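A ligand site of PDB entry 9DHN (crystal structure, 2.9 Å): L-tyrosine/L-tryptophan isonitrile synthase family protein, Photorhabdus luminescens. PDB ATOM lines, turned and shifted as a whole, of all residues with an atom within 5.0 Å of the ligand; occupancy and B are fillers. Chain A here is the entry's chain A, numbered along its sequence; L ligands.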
ATOM      1  N   PRO A  64      -7.288  33.358  17.224  1.00  0.00           N
ATOM      2  CA  PRO A  64      -8.423  32.819  16.472  1.00  0.00           C
ATOM      3  C   PRO A  64      -9.339  31.833  17.200  1.00  0.00           C
ATOM      4  O   PRO A  64     -10.528  32.020  17.145  1.00  0.00           O
ATOM      5  CB  PRO A  64      -7.699  31.945  15.436  1.00  0.00           C
ATOM      6  CG  PRO A  64      -6.366  31.605  16.040  1.00  0.00           C
ATOM      7  CD  PRO A  64      -5.989  32.857  16.787  1.00  0.00           C
ATOM      8  N   THR A  65      -8.772  30.857  17.909  1.00  0.00           N
ATOM      9  CA  THR A  65      -9.560  29.863  18.682  1.00  0.00           C
ATOM     10  C   THR A  65      -8.620  29.175  19.671  1.00  0.00           C
ATOM     11  O   THR A  65      -7.410  29.270  19.475  1.00  0.00           O
ATOM     12  CB  THR A  65     -10.265  28.846  17.786  1.00  0.00           C
ATOM     13  OG1 THR A  65     -11.099  28.058  18.634  1.00  0.00           O
ATOM     14  CG2 THR A  65      -9.300  27.957  17.022  1.00  0.00           C
ATOM     15  N   LYS A  66      -9.170  28.492  20.665  1.00  0.00           N
ATOM     16  CA  LYS A  66      -8.289  27.711  21.569  1.00  0.00           C
ATOM     17  C   LYS A  66      -7.930  26.375  20.923  1.00  0.00           C
ATOM     18  O   LYS A  66      -8.794  25.806  20.233  1.00  0.00           O
ATOM     19  CB  LYS A  66      -8.963  27.462  22.912  1.00  0.00           C
ATOM     20  CG  LYS A  66      -8.008  27.157  24.063  1.00  0.00           C
ATOM     21  CD  LYS A  66      -7.199  28.354  24.482  1.00  0.00           C
ATOM     22  CE  LYS A  66      -6.386  28.100  25.739  1.00  0.00           C
ATOM     23  NZ  LYS A  66      -5.583  29.276  26.121  1.00  0.00           N
ATOM     24  N   SER A  67      -6.711  25.907  21.132  1.00  0.00           N
ATOM     25  CA  SER A  67      -6.263  24.655  20.531  1.00  0.00           C
ATOM     26  C   SER A  67      -7.030  23.470  21.091  1.00  0.00           C
ATOM     27  O   SER A  67      -7.194  23.357  22.314  1.00  0.00           O
ATOM     28  CB  SER A  67      -4.785  24.404  20.781  1.00  0.00           C
ATOM     29  OG  SER A  67      -4.403  23.167  20.214  1.00  0.00           O
ATOM     30  N   PRO A  68      -7.447  22.528  20.242  1.00  0.00           N
ATOM     31  CA  PRO A  68      -8.293  21.434  20.726  1.00  0.00           C
ATOM     32  C   PRO A  68      -7.513  20.350  21.468  1.00  0.00           C
ATOM     33  O   PRO A  68      -8.124  19.595  22.239  1.00  0.00           O
ATOM     34  CB  PRO A  68      -8.972  20.882  19.479  1.00  0.00           C
ATOM     35  CG  PRO A  68      -8.026  21.236  18.333  1.00  0.00           C
ATOM     36  CD  PRO A  68      -7.290  22.469  18.724  1.00  0.00           C
ATOM     37  N   ASP A 111      -8.364  35.794  13.579  1.00  0.00           N
ATOM     38  CA  ASP A 111      -8.413  35.024  12.344  1.00  0.00           C
ATOM     39  C   ASP A 111      -9.158  33.695  12.523  1.00  0.00           C
ATOM     40  O   ASP A 111      -8.851  32.720  11.813  1.00  0.00           O
ATOM     41  CB  ASP A 111      -7.005  34.791  11.792  1.00  0.00           C
ATOM     42  CG  ASP A 111      -5.962  34.483  12.865  1.00  0.00           C
ATOM     43  OD1 ASP A 111      -6.273  34.584  14.066  1.00  0.00           O
ATOM     44  OD2 ASP A 111      -4.821  34.147  12.503  1.00  0.00           O
ATOM     45  N   PHE A 115      -9.658  30.059   8.931  1.00  0.00           N
ATOM     46  CA  PHE A 115      -9.169  28.704   8.725  1.00  0.00           C
ATOM     47  C   PHE A 115      -9.886  27.675   9.591  1.00  0.00           C
ATOM     48  O   PHE A 115      -9.385  26.554   9.749  1.00  0.00           O
ATOM     49  CB  PHE A 115      -7.647  28.635   8.861  1.00  0.00           C
ATOM     50  CG  PHE A 115      -7.086  29.379  10.045  1.00  0.00           C
ATOM     51  CD1 PHE A 115      -7.487  29.064  11.339  1.00  0.00           C
ATOM     52  CD2 PHE A 115      -6.105  30.339   9.869  1.00  0.00           C
ATOM     53  CE1 PHE A 115      -6.950  29.709  12.444  1.00  0.00           C
ATOM     54  CE2 PHE A 115      -5.574  31.005  10.971  1.00  0.00           C
ATOM     55  CZ  PHE A 115      -5.981  30.683  12.261  1.00  0.00           C
ATOM     56  N   ILE A 119      -8.637  23.654  10.795  1.00  0.00           N
ATOM     57  CA  ILE A 119      -8.256  23.248  12.145  1.00  0.00           C
ATOM     58  C   ILE A 119      -9.160  22.155  12.678  1.00  0.00           C
ATOM     59  O   ILE A 119      -8.797  21.493  13.661  1.00  0.00           O
ATOM     60  CB  ILE A 119      -8.399  24.365  13.186  1.00  0.00           C
ATOM     61  CG1 ILE A 119      -8.208  25.732  12.585  1.00  0.00           C
ATOM     62  CG2 ILE A 119      -7.435  24.116  14.319  1.00  0.00           C
ATOM     63  CD1 ILE A 119      -8.563  26.794  13.574  1.00  0.00           C
ATOM     64  N   VAL A 121     -12.294  22.683  13.876  1.00  0.00           N
ATOM     65  CA  VAL A 121     -12.789  23.302  15.145  1.00  0.00           C
ATOM     66  C   VAL A 121     -14.150  23.870  14.750  1.00  0.00           C
ATOM     67  O   VAL A 121     -14.231  24.522  13.699  1.00  0.00           O
ATOM     68  CB  VAL A 121     -11.880  24.358  15.798  1.00  0.00           C
ATOM     69  CG1 VAL A 121     -12.591  25.078  16.932  1.00  0.00           C
ATOM     70  CG2 VAL A 121     -10.587  23.749  16.294  1.00  0.00           C
ATOM     71  N   LEU A 194       8.429  28.558   8.914  1.00  0.00           N
ATOM     72  CA  LEU A 194       6.998  28.755   9.128  1.00  0.00           C
ATOM     73  C   LEU A 194       6.231  27.494   8.765  1.00  0.00           C
ATOM     74  O   LEU A 194       5.375  27.024   9.520  1.00  0.00           O
ATOM     75  CB  LEU A 194       6.531  29.943   8.289  1.00  0.00           C
ATOM     76  CG  LEU A 194       5.029  30.159   8.162  1.00  0.00           C
ATOM     77  CD1 LEU A 194       4.477  30.602   9.493  1.00  0.00           C
ATOM     78  CD2 LEU A 194       4.740  31.174   7.101  1.00  0.00           C
ATOM     79  N   ALA A 197       6.745  24.837  11.355  1.00  0.00           N
ATOM     80  CA  ALA A 197       6.056  25.118  12.595  1.00  0.00           C
ATOM     81  C   ALA A 197       4.561  24.847  12.465  1.00  0.00           C
ATOM     82  O   ALA A 197       3.972  24.157  13.303  1.00  0.00           O
ATOM     83  CB  ALA A 197       6.300  26.561  13.000  1.00  0.00           C
ATOM     84  N   VAL A 198       3.962  25.327  11.383  1.00  0.00           N
ATOM     85  CA  VAL A 198       2.517  25.183  11.188  1.00  0.00           C
ATOM     86  C   VAL A 198       2.133  23.721  11.037  1.00  0.00           C
ATOM     87  O   VAL A 198       1.085  23.287  11.534  1.00  0.00           O
ATOM     88  CB  VAL A 198       2.070  26.043  10.002  1.00  0.00           C
ATOM     89  CG1 VAL A 198       0.691  25.649   9.539  1.00  0.00           C
ATOM     90  CG2 VAL A 198       2.139  27.515  10.406  1.00  0.00           C
ATOM     91  N   PHE A 201       2.235  22.128  14.665  1.00  0.00           N
ATOM     92  CA  PHE A 201       1.070  22.446  15.488  1.00  0.00           C
ATOM     93  C   PHE A 201      -0.166  21.697  14.990  1.00  0.00           C
ATOM     94  O   PHE A 201      -0.956  21.213  15.802  1.00  0.00           O
ATOM     95  CB  PHE A 201       0.833  23.961  15.531  1.00  0.00           C
ATOM     96  CG  PHE A 201       1.774  24.687  16.473  1.00  0.00           C
ATOM     97  CD1 PHE A 201       1.882  24.297  17.828  1.00  0.00           C
ATOM     98  CD2 PHE A 201       2.566  25.732  16.017  1.00  0.00           C
ATOM     99  CE1 PHE A 201       2.763  24.959  18.718  1.00  0.00           C
ATOM    100  CE2 PHE A 201       3.462  26.386  16.892  1.00  0.00           C
ATOM    101  CZ  PHE A 201       3.553  25.997  18.250  1.00  0.00           C
ATOM    102  N   LEU A 202      -0.326  21.564  13.669  1.00  0.00           N
ATOM    103  CA  LEU A 202      -1.496  20.857  13.137  1.00  0.00           C
ATOM    104  C   LEU A 202      -1.417  19.358  13.429  1.00  0.00           C
ATOM    105  O   LEU A 202      -2.430  18.725  13.733  1.00  0.00           O
ATOM    106  CB  LEU A 202      -1.643  21.090  11.640  1.00  0.00           C
ATOM    107  CG  LEU A 202      -1.989  22.519  11.187  1.00  0.00           C
ATOM    108  CD1 LEU A 202      -2.332  22.578   9.714  1.00  0.00           C
ATOM    109  CD2 LEU A 202      -3.149  23.049  12.001  1.00  0.00           C
ATOM    110  N   ASP A 205      -2.257  18.721  17.348  1.00  0.00           N
ATOM    111  CA  ASP A 205      -3.673  18.792  17.683  1.00  0.00           C
ATOM    112  C   ASP A 205      -4.468  17.622  17.147  1.00  0.00           C
ATOM    113  O   ASP A 205      -5.575  17.372  17.635  1.00  0.00           O
ATOM    114  CB  ASP A 205      -4.296  20.095  17.179  1.00  0.00           C
ATOM    115  CG  ASP A 205      -3.544  21.279  17.647  1.00  0.00           C
ATOM    116  OD1 ASP A 205      -2.468  21.047  18.241  1.00  0.00           O
ATOM    117  OD2 ASP A 205      -4.007  22.421  17.430  1.00  0.00           O
ATOM    118  N   VAL A 229      -3.773  26.316   5.710  1.00  0.00           N
ATOM    119  CA  VAL A 229      -3.937  27.285   6.775  1.00  0.00           C
ATOM    120  C   VAL A 229      -3.120  28.528   6.488  1.00  0.00           C
ATOM    121  O   VAL A 229      -3.563  29.658   6.755  1.00  0.00           O
ATOM    122  CB  VAL A 229      -3.551  26.674   8.130  1.00  0.00           C
ATOM    123  CG1 VAL A 229      -3.132  27.764   9.114  1.00  0.00           C
ATOM    124  CG2 VAL A 229      -4.694  25.915   8.683  1.00  0.00           C
ATOM    125  N   ILE A 230      -1.905  28.367   5.971  1.00  0.00           N
ATOM    126  CA  ILE A 230      -1.110  29.532   5.617  1.00  0.00           C
ATOM    127  C   ILE A 230      -1.776  30.317   4.498  1.00  0.00           C
ATOM    128  O   ILE A 230      -1.777  31.554   4.497  1.00  0.00           O
ATOM    129  CB  ILE A 230       0.322  29.151   5.248  1.00  0.00           C
ATOM    130  CG1 ILE A 230       1.054  28.691   6.488  1.00  0.00           C
ATOM    131  CG2 ILE A 230       1.033  30.372   4.748  1.00  0.00           C
ATOM    132  CD1 ILE A 230       2.223  27.817   6.190  1.00  0.00           C
ATOM    133  N   SER A 233      -4.503  32.335   6.016  1.00  0.00           N
ATOM    134  CA  SER A 233      -4.032  33.424   6.870  1.00  0.00           C
ATOM    135  C   SER A 233      -3.357  34.532   6.071  1.00  0.00           C
ATOM    136  O   SER A 233      -3.462  35.701   6.456  1.00  0.00           O
ATOM    137  CB  SER A 233      -3.101  32.892   7.943  1.00  0.00           C
ATOM    138  OG  SER A 233      -3.188  33.747   9.072  1.00  0.00           O
ATOM    139  N   ILE A 252       2.074  37.477  15.233  1.00  0.00           N
ATOM    140  CA  ILE A 252       2.226  36.520  16.312  1.00  0.00           C
ATOM    141  C   ILE A 252       3.264  35.456  16.004  1.00  0.00           C
ATOM    142  O   ILE A 252       3.549  34.610  16.858  1.00  0.00           O
ATOM    143  CB  ILE A 252       0.837  35.932  16.634  1.00  0.00           C
ATOM    144  CG1 ILE A 252       0.728  35.771  18.133  1.00  0.00           C
ATOM    145  CG2 ILE A 252       0.558  34.643  15.837  1.00  0.00           C
ATOM    146  CD1 ILE A 252       0.825  37.125  18.869  1.00  0.00           C
ATOM    147  N   HIS A 253       3.868  35.487  14.807  1.00  0.00           N
ATOM    148  CA  HIS A 253       4.927  34.655  14.261  1.00  0.00           C
ATOM    149  C   HIS A 253       6.251  35.393  14.174  1.00  0.00           C
ATOM    150  O   HIS A 253       6.273  36.601  13.914  1.00  0.00           O
ATOM    151  CB  HIS A 253       4.593  34.183  12.842  1.00  0.00           C
ATOM    152  CG  HIS A 253       3.295  33.486  12.727  1.00  0.00           C
ATOM    153  ND1 HIS A 253       2.405  33.757  11.712  1.00  0.00           N
ATOM    154  CD2 HIS A 253       2.727  32.526  13.490  1.00  0.00           C
ATOM    155  CE1 HIS A 253       1.350  32.996  11.848  1.00  0.00           C
ATOM    156  NE2 HIS A 253       1.516  32.237  12.933  1.00  0.00           N
ATOM    157  N   TRP A 273       7.419  30.274  18.872  1.00  0.00           N
ATOM    158  CA  TRP A 273       6.163  30.013  18.190  1.00  0.00           C
ATOM    159  C   TRP A 273       4.986  29.844  19.136  1.00  0.00           C
ATOM    160  O   TRP A 273       3.854  29.681  18.675  1.00  0.00           O
ATOM    161  CB  TRP A 273       6.286  28.748  17.353  1.00  0.00           C
ATOM    162  CG  TRP A 273       7.219  28.912  16.247  1.00  0.00           C
ATOM    163  CD1 TRP A 273       8.512  28.554  16.222  1.00  0.00           C
ATOM    164  CD2 TRP A 273       6.937  29.494  14.969  1.00  0.00           C
ATOM    165  NE1 TRP A 273       9.077  28.868  15.014  1.00  0.00           N
ATOM    166  CE2 TRP A 273       8.117  29.452  14.229  1.00  0.00           C
ATOM    167  CE3 TRP A 273       5.790  30.066  14.392  1.00  0.00           C
ATOM    168  CZ2 TRP A 273       8.204  29.953  12.929  1.00  0.00           C
ATOM    169  CZ3 TRP A 273       5.868  30.554  13.109  1.00  0.00           C
ATOM    170  CH2 TRP A 273       7.057  30.490  12.397  1.00  0.00           C
ATOM    171  N   TRP A 277      -3.119  30.758  22.845  1.00  0.00           N
ATOM    172  CA  TRP A 277      -4.175  29.811  22.520  1.00  0.00           C
ATOM    173  C   TRP A 277      -3.636  28.426  22.250  1.00  0.00           C
ATOM    174  O   TRP A 277      -4.412  27.525  21.924  1.00  0.00           O
ATOM    175  CB  TRP A 277      -5.014  30.320  21.348  1.00  0.00           C
ATOM    176  CG  TRP A 277      -4.228  30.831  20.174  1.00  0.00           C
ATOM    177  CD1 TRP A 277      -3.940  30.165  19.012  1.00  0.00           C
ATOM    178  CD2 TRP A 277      -3.634  32.133  20.041  1.00  0.00           C
ATOM    179  NE1 TRP A 277      -3.204  30.967  18.169  1.00  0.00           N
ATOM    180  CE2 TRP A 277      -2.997  32.178  18.783  1.00  0.00           C
ATOM    181  CE3 TRP A 277      -3.579  33.255  20.870  1.00  0.00           C
ATOM    182  CZ2 TRP A 277      -2.303  33.308  18.332  1.00  0.00           C
ATOM    183  CZ3 TRP A 277      -2.886  34.371  20.419  1.00  0.00           C
ATOM    184  CH2 TRP A 277      -2.272  34.394  19.160  1.00  0.00           C
ATOM    185  N   HIS A 278      -2.319  28.225  22.394  1.00  0.00           N
ATOM    186  CA  HIS A 278      -1.709  26.918  22.249  1.00  0.00           C
ATOM    187  C   HIS A 278      -0.951  26.501  23.502  1.00  0.00           C
ATOM    188  O   HIS A 278      -0.042  25.658  23.430  1.00  0.00           O
ATOM    189  CB  HIS A 278      -0.782  26.896  21.029  1.00  0.00           C
ATOM    190  CG  HIS A 278      -1.491  27.051  19.725  1.00  0.00           C
ATOM    191  ND1 HIS A 278      -2.360  26.094  19.240  1.00  0.00           N
ATOM    192  CD2 HIS A 278      -1.492  28.050  18.815  1.00  0.00           C
ATOM    193  CE1 HIS A 278      -2.866  26.509  18.084  1.00  0.00           C
ATOM    194  NE2 HIS A 278      -2.351  27.691  17.810  1.00  0.00           N
HETATM  195  C1  LIG L   1      -3.867  26.112  14.955  1.00  0.00           C
HETATM  196  C2  LIG L   1       0.016  31.094   9.745  1.00  0.00           C
HETATM  197  C3  LIG L   1      -1.116  30.712  10.727  1.00  0.00           C
HETATM  198  C4  LIG L   1      -0.870  30.124  12.122  1.00  0.00           C
HETATM  199  C5  LIG L   1      -1.792  30.675  13.261  1.00  0.00           C
HETATM  200  C6  LIG L   1      -2.013  32.204  13.211  1.00  0.00           C
HETATM  201  C7  LIG L   1      -3.649  27.474  14.841  1.00  0.00           C
HETATM  202  C8  LIG L   1      -4.852  25.622  15.790  1.00  0.00           C
HETATM  203  C9  LIG L   1      -5.651  26.489  16.528  1.00  0.00           C
HETATM  204  C10 LIG L   1      -4.436  28.340  15.585  1.00  0.00           C
HETATM  205  C11 LIG L   1      -0.059  28.037  14.590  1.00  0.00           C
HETATM  206  O1  LIG L   1      -3.205  32.528  13.885  1.00  0.00           O
HETATM  207  O2  LIG L   1       1.032  28.665  14.766  1.00  0.00           O
HETATM  208  C12 LIG L   1      -1.448  28.707  14.742  1.00  0.00           C
HETATM  209  C13 LIG L   1      -2.533  27.976  13.939  1.00  0.00           C
HETATM  210  C14 LIG L   1      -5.444  27.858  16.419  1.00  0.00           C
HETATM  211  N1  LIG L   1      -1.480  30.184  14.621  1.00  0.00           N
HETATM  212  O3  LIG L   1      -2.244  30.854  10.400  1.00  0.00           O
HETATM  213  O4  LIG L   1       0.499  30.086  12.460  1.00  0.00           O
HETATM  214  O5  LIG L   1      -6.662  25.943  17.349  1.00  0.00           O
HETATM  215  O6  LIG L   1      -0.017  26.797  14.297  1.00  0.00           O
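O4 of the ligand lies within hydrogen-bond range of NE2 of His 253 (2.4 Å). O1 of the ligand sits at hydrogen-bond distance from OD2 of Asp 111. An oxygen (O3) of the ligand sits close to the side-chain hydroxyl of Ser 233 (3.3 Å).
A ring nitrogen (NE2) of His 278 sits close to the indole nitrogen (NE1) of Trp 277, at 3.4 Å. The side-chain hydroxyl (OG) of Ser 67 sits at hydrogen-bond distance from the side-chain carboxylate (OD2) of Asp 205 (2.9 Å). The backbone NH of Ser 67 sits at hydrogen-bond distance from the backbone carbonyl oxygen of Trp 277 (2.9 Å).
CG of Pro 64 touches C10 of the ligand (3.8 Å). CG2 of Thr 65 touches O5 of the ligand, at 3.3 Å. O of Lys 66 touches O5 of the ligand (3.6 Å). Ser 67 touches the ligand. Pro 68 touches the ligand. Phe 115 touches the ligand (CE2 to O3, 3.4 Å). CG2 of Ile 119 touches C8 of the ligand, 3.3 Å away. Val 198 touches the ligand. CB of Phe 201 touches O6 of the ligand, at 3.2 Å. Asp 205 touches the ligand. Val 229 touches the ligand (CG1 to O3, 3.5 Å). CD1 of Trp 277 touches C14 of the ligand, at 3.8 Å. His 278 touches the ligand (NE2 to C10, 3.1 Å). Hydrophobic or aromatic side chains that line the ligand: Pro 64, Pro 68, Phe 115, Ile 119, Val 198, Phe 201, Val 229, His 253, Trp 277 and His 278. Of the 23 residues printed, 16 come within 4 Å of the ligand. The nearest printed residue that does not touch the ligand is Ile 230 (4.2 Å).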
